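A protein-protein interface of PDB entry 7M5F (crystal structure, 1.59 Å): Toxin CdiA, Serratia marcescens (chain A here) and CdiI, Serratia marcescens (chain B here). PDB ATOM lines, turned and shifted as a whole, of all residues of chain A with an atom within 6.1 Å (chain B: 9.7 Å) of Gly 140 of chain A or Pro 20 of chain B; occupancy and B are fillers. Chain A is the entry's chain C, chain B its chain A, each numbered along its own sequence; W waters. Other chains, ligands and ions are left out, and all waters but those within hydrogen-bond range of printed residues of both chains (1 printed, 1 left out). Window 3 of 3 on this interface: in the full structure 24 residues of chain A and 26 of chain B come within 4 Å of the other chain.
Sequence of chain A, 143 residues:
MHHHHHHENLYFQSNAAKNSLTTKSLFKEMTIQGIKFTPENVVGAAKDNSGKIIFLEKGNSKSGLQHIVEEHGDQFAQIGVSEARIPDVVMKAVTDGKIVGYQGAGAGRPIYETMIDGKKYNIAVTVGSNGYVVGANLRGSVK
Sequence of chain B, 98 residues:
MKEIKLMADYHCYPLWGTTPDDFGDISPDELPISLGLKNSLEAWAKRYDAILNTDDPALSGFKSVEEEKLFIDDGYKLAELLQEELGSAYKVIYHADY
The side-chain carboxylate of Asp 25 of chain B is in salt-bridge range of the guanidinium group of Arg 139 of chain A (2.8 Å). O of Phe 23 of chain B lies within hydrogen-bond range of N of Gly 140 of chain A, 2.9 Å away. O of Thr 18 of chain B lies within hydrogen-bond range of NE2 of Gln 78 of chain A (3.0 Å).
The side-chain carboxylate of Asp 22 of chain B lies within hydrogen-bond range of the backbone NH of Thr 18 of chain B (3.2 Å). N of Gly 17 of chain B sits at hydrogen-bond distance from O of Gly 24 of chain B. The backbone NH of Arg 139 of chain A lies within hydrogen-bond range of the backbone carbonyl oxygen of Asn 122 of chain A (2.9 Å).
Gln 78 of chain A touches Pro 20 of chain B. Gln 78 of chain A touches Phe 23 of chain B. Phe 23 of chain B touches Leu 138 of chain A (CB to O, 3.7 Å). Leu 138 of chain A touches Gly 24 of chain B. Arg 139 of chain A touches Phe 23 of chain B. NH1 of Arg 139 of chain A touches CA of Gly 24 of chain B, 3.7 Å away. Gly 140 of chain A touches Pro 20 of chain B (CA to O, 3.6 Å).
Gly 140 of chain A touches two residues of chain B. Printed residues of chain A within 4 Å of Asp 25 of chain B: Arg 139 (2.8 Å). Of the printed residues of chain B, Gln 78 of chain A touches Thr 18, Pro 20 and Phe 23. Of the printed residues of chain B, Arg 139 of chain A touches Phe 23, Gly 24 and Asp 25. The nearest residue of chain B that does not touch Gly 140 of chain A is Asp 21 of chain B (4.1 Å). The nearest residue of chain A that does not touch Pro 20 of chain B is Ile 79 of chain A (4.6 Å).
Along chain A the printed residues that touch a printed residue of chain B span positions 78 to 140. Of the 11 printed residues of chain B, 5 touch a printed residue of chain A. Hydrophobic or aromatic side chains of chain B within 4 Å of the printed part of chain A: Pro 20 and Phe 23.
Water W1 bridges OE1 of Gln 78 of chain A and O of Thr 18 of chain B.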
ATOM      1  N   GLN A  78     -11.265 -11.444   3.196  1.00  0.00           N
ATOM      2  CA  GLN A  78     -10.508 -12.611   3.605  1.00  0.00           C
ATOM      3  C   GLN A  78      -9.001 -12.377   3.652  1.00  0.00           C
ATOM      4  O   GLN A  78      -8.314 -13.097   4.378  1.00  0.00           O
ATOM      5  CB  GLN A  78     -10.811 -13.793   2.670  1.00  0.00           C
ATOM      6  CG  GLN A  78     -12.199 -14.396   2.812  1.00  0.00           C
ATOM      7  CD  GLN A  78     -12.345 -15.731   2.087  1.00  0.00           C
ATOM      8  OE1 GLN A  78     -11.648 -16.697   2.396  1.00  0.00           O
ATOM      9  NE2 GLN A  78     -13.249 -15.782   1.121  1.00  0.00           N
ATOM     10  N   ILE A  79      -8.457 -11.408   2.917  1.00  0.00           N
ATOM     11  CA  ILE A  79      -7.030 -11.125   2.997  1.00  0.00           C
ATOM     12  C   ILE A  79      -6.750  -9.924   3.893  1.00  0.00           C
ATOM     13  O   ILE A  79      -5.630  -9.406   3.893  1.00  0.00           O
ATOM     14  CB  ILE A  79      -6.377 -10.916   1.619  1.00  0.00           C
ATOM     15  CG1 ILE A  79      -6.909  -9.666   0.928  1.00  0.00           C
ATOM     16  CG2 ILE A  79      -6.589 -12.150   0.729  1.00  0.00           C
ATOM     17  CD1 ILE A  79      -5.925  -9.041  -0.048  1.00  0.00           C
ATOM     18  N   ASN A 122      -1.762 -10.634  -6.737  1.00  0.00           N
ATOM     19  CA  ASN A 122      -2.219 -10.426  -8.103  1.00  0.00           C
ATOM     20  C   ASN A 122      -3.661  -9.946  -8.098  1.00  0.00           C
ATOM     21  O   ASN A 122      -4.531 -10.574  -7.478  1.00  0.00           O
ATOM     22  CB  ASN A 122      -2.104 -11.708  -8.933  1.00  0.00           C
ATOM     23  CG  ASN A 122      -0.654 -12.121  -9.228  1.00  0.00           C
ATOM     24  OD1 ASN A 122       0.286 -11.335  -9.140  1.00  0.00           O
ATOM     25  ND2 ASN A 122      -0.486 -13.372  -9.614  1.00  0.00           N
ATOM     26  N   LEU A 138      -9.262 -10.262  -6.928  1.00  0.00           N
ATOM     27  CA  LEU A 138      -8.014 -10.870  -6.488  1.00  0.00           C
ATOM     28  C   LEU A 138      -7.822 -12.240  -7.136  1.00  0.00           C
ATOM     29  O   LEU A 138      -8.777 -12.908  -7.548  1.00  0.00           O
ATOM     30  CB  LEU A 138      -7.990 -11.012  -4.967  1.00  0.00           C
ATOM     31  CG  LEU A 138      -7.706  -9.734  -4.187  1.00  0.00           C
ATOM     32  CD1 LEU A 138      -8.236  -9.874  -2.787  1.00  0.00           C
ATOM     33  CD2 LEU A 138      -6.182  -9.541  -4.173  1.00  0.00           C
ATOM     34  N   ARG A 139      -6.566 -12.670  -7.185  1.00  0.00           N
ATOM     35  CA  ARG A 139      -6.228 -14.024  -7.577  1.00  0.00           C
ATOM     36  C   ARG A 139      -5.409 -14.661  -6.471  1.00  0.00           C
ATOM     37  O   ARG A 139      -4.907 -13.985  -5.568  1.00  0.00           O
ATOM     38  CB  ARG A 139      -5.442 -14.054  -8.881  1.00  0.00           C
ATOM     39  CG  ARG A 139      -6.244 -13.813 -10.103  1.00  0.00           C
ATOM     40  CD  ARG A 139      -5.489 -14.300 -11.357  1.00  0.00           C
ATOM     41  NE  ARG A 139      -5.474 -15.732 -11.563  1.00  0.00           N
ATOM     42  CZ  ARG A 139      -6.459 -16.452 -12.098  1.00  0.00           C
ATOM     43  NH1 ARG A 139      -7.583 -15.879 -12.471  1.00  0.00           N
ATOM     44  NH2 ARG A 139      -6.327 -17.767 -12.244  1.00  0.00           N
ATOM     45  N   GLY A 140      -5.271 -15.978  -6.542  1.00  0.00           N
ATOM     46  CA  GLY A 140      -4.381 -16.680  -5.643  1.00  0.00           C
ATOM     47  C   GLY A 140      -2.970 -16.682  -6.197  1.00  0.00           C
ATOM     48  O   GLY A 140      -2.743 -16.234  -7.327  1.00  0.00           O
ATOM     49  N   TRP B  16     -15.659 -19.213  -9.996  1.00  0.00           N
ATOM     50  CA  TRP B  16     -14.704 -18.580  -9.093  1.00  0.00           C
ATOM     51  C   TRP B  16     -14.378 -19.449  -7.892  1.00  0.00           C
ATOM     52  O   TRP B  16     -15.261 -20.088  -7.320  1.00  0.00           O
ATOM     53  CB  TRP B  16     -15.250 -17.219  -8.581  1.00  0.00           C
ATOM     54  CG  TRP B  16     -15.569 -16.288  -9.690  1.00  0.00           C
ATOM     55  CD1 TRP B  16     -16.722 -16.254 -10.411  1.00  0.00           C
ATOM     56  CD2 TRP B  16     -14.712 -15.294 -10.253  1.00  0.00           C
ATOM     57  NE1 TRP B  16     -16.637 -15.306 -11.375  1.00  0.00           N
ATOM     58  CE2 TRP B  16     -15.414 -14.694 -11.307  1.00  0.00           C
ATOM     59  CE3 TRP B  16     -13.412 -14.862  -9.964  1.00  0.00           C
ATOM     60  CZ2 TRP B  16     -14.875 -13.654 -12.079  1.00  0.00           C
ATOM     61  CZ3 TRP B  16     -12.862 -13.838 -10.739  1.00  0.00           C
ATOM     62  CH2 TRP B  16     -13.603 -13.247 -11.781  1.00  0.00           C
ATOM     63  N   GLY B  17     -13.100 -19.445  -7.494  1.00  0.00           N
ATOM     64  CA  GLY B  17     -12.722 -20.010  -6.216  1.00  0.00           C
ATOM     65  C   GLY B  17     -13.033 -19.065  -5.086  1.00  0.00           C
ATOM     66  O   GLY B  17     -13.152 -17.853  -5.294  1.00  0.00           O
ATOM     67  N   THR B  18     -13.222 -19.613  -3.887  1.00  0.00           N
ATOM     68  CA  THR B  18     -13.696 -18.793  -2.777  1.00  0.00           C
ATOM     69  C   THR B  18     -12.784 -18.783  -1.572  1.00  0.00           C
ATOM     70  O   THR B  18     -13.184 -18.259  -0.520  1.00  0.00           O
ATOM     71  CB  THR B  18     -15.096 -19.227  -2.332  1.00  0.00           C
ATOM     72  OG1 THR B  18     -15.003 -20.507  -1.711  1.00  0.00           O
ATOM     73  CG2 THR B  18     -16.044 -19.257  -3.492  1.00  0.00           C
ATOM     74  N   THR B  19     -11.572 -19.333  -1.669  1.00  0.00           N
ATOM     75  CA  THR B  19     -10.586 -19.267  -0.608  1.00  0.00           C
ATOM     76  C   THR B  19      -9.339 -18.568  -1.119  1.00  0.00           C
ATOM     77  O   THR B  19      -9.087 -18.541  -2.330  1.00  0.00           O
ATOM     78  CB  THR B  19     -10.200 -20.661  -0.100  1.00  0.00           C
ATOM     79  OG1 THR B  19      -9.343 -21.289  -1.062  1.00  0.00           O
ATOM     80  CG2 THR B  19     -11.421 -21.506   0.136  1.00  0.00           C
ATOM     81  N   PRO B  20      -8.545 -17.969  -0.227  1.00  0.00           N
ATOM     82  CA  PRO B  20      -7.368 -17.229  -0.703  1.00  0.00           C
ATOM     83  C   PRO B  20      -6.430 -18.062  -1.558  1.00  0.00           C
ATOM     84  O   PRO B  20      -5.838 -17.533  -2.508  1.00  0.00           O
ATOM     85  CB  PRO B  20      -6.704 -16.761   0.596  1.00  0.00           C
ATOM     86  CG  PRO B  20      -7.851 -16.640   1.570  1.00  0.00           C
ATOM     87  CD  PRO B  20      -8.785 -17.779   1.212  1.00  0.00           C
ATOM     88  N   ASP B  21      -6.307 -19.362  -1.292  1.00  0.00           N
ATOM     89  CA  ASP B  21      -5.434 -20.185  -2.118  1.00  0.00           C
ATOM     90  C   ASP B  21      -5.933 -20.329  -3.554  1.00  0.00           C
ATOM     91  O   ASP B  21      -5.123 -20.567  -4.457  1.00  0.00           O
ATOM     92  CB  ASP B  21      -5.293 -21.570  -1.496  1.00  0.00           C
ATOM     93  CG  ASP B  21      -4.401 -21.569  -0.278  1.00  0.00           C
ATOM     94  OD1 ASP B  21      -3.519 -20.689  -0.197  1.00  0.00           O
ATOM     95  OD2 ASP B  21      -4.579 -22.450   0.592  1.00  0.00           O
ATOM     96  N   ASP B  22      -7.244 -20.219  -3.802  1.00  0.00           N
ATOM     97  CA  ASP B  22      -7.764 -20.451  -5.149  1.00  0.00           C
ATOM     98  C   ASP B  22      -8.628 -19.300  -5.668  1.00  0.00           C
ATOM     99  O   ASP B  22      -9.431 -19.487  -6.591  1.00  0.00           O
ATOM    100  CB  ASP B  22      -8.524 -21.784  -5.221  1.00  0.00           C
ATOM    101  CG  ASP B  22      -9.895 -21.747  -4.551  1.00  0.00           C
ATOM    102  OD1 ASP B  22     -10.232 -20.780  -3.861  1.00  0.00           O
ATOM    103  OD2 ASP B  22     -10.663 -22.718  -4.745  1.00  0.00           O
ATOM    104  N   PHE B  23      -8.443 -18.089  -5.148  1.00  0.00           N
ATOM    105  CA  PHE B  23      -9.123 -16.940  -5.706  1.00  0.00           C
ATOM    106  C   PHE B  23      -8.815 -16.819  -7.197  1.00  0.00           C
ATOM    107  O   PHE B  23      -7.702 -17.157  -7.652  1.00  0.00           O
ATOM    108  CB  PHE B  23      -8.693 -15.644  -5.030  1.00  0.00           C
ATOM    109  CG  PHE B  23      -9.326 -15.388  -3.677  1.00  0.00           C
ATOM    110  CD1 PHE B  23     -10.549 -15.912  -3.337  1.00  0.00           C
ATOM    111  CD2 PHE B  23      -8.682 -14.578  -2.765  1.00  0.00           C
ATOM    112  CE1 PHE B  23     -11.105 -15.636  -2.100  1.00  0.00           C
ATOM    113  CE2 PHE B  23      -9.251 -14.308  -1.545  1.00  0.00           C
ATOM    114  CZ  PHE B  23     -10.479 -14.855  -1.240  1.00  0.00           C
ATOM    115  N   GLY B  24      -9.790 -16.324  -7.939  1.00  0.00           N
ATOM    116  CA  GLY B  24      -9.669 -16.110  -9.370  1.00  0.00           C
ATOM    117  C   GLY B  24     -10.687 -16.925 -10.149  1.00  0.00           C
ATOM    118  O   GLY B  24     -11.400 -17.768  -9.610  1.00  0.00           O
ATOM    119  N   ASP B  25     -10.767 -16.627 -11.440  1.00  0.00           N
ATOM    120  CA  ASP B  25     -11.726 -17.343 -12.268  1.00  0.00           C
ATOM    121  C   ASP B  25     -11.175 -18.716 -12.649  1.00  0.00           C
ATOM    122  O   ASP B  25      -9.970 -19.002 -12.551  1.00  0.00           O
ATOM    123  CB  ASP B  25     -12.153 -16.509 -13.491  1.00  0.00           C
ATOM    124  CG  ASP B  25     -11.041 -16.241 -14.488  1.00  0.00           C
ATOM    125  OD1 ASP B  25      -9.846 -16.283 -14.136  1.00  0.00           O
ATOM    126  OD2 ASP B  25     -11.372 -15.913 -15.649  1.00  0.00           O
ATOM    127  N   ILE B  26     -12.102 -19.597 -13.021  1.00  0.00           N
ATOM    128  CA  ILE B  26     -11.839 -21.010 -13.256  1.00  0.00           C
ATOM    129  C   ILE B  26     -12.460 -21.369 -14.602  1.00  0.00           C
ATOM    130  O   ILE B  26     -13.654 -21.154 -14.816  1.00  0.00           O
ATOM    131  CB  ILE B  26     -12.446 -21.892 -12.150  1.00  0.00           C
ATOM    132  CG1 ILE B  26     -11.851 -21.575 -10.779  1.00  0.00           C
ATOM    133  CG2 ILE B  26     -12.197 -23.361 -12.467  1.00  0.00           C
ATOM    134  CD1 ILE B  26     -12.551 -22.250  -9.615  1.00  0.00           C
HETATM  135  O   HOH W   1     -12.735 -19.151   2.653  1.00  0.00           O
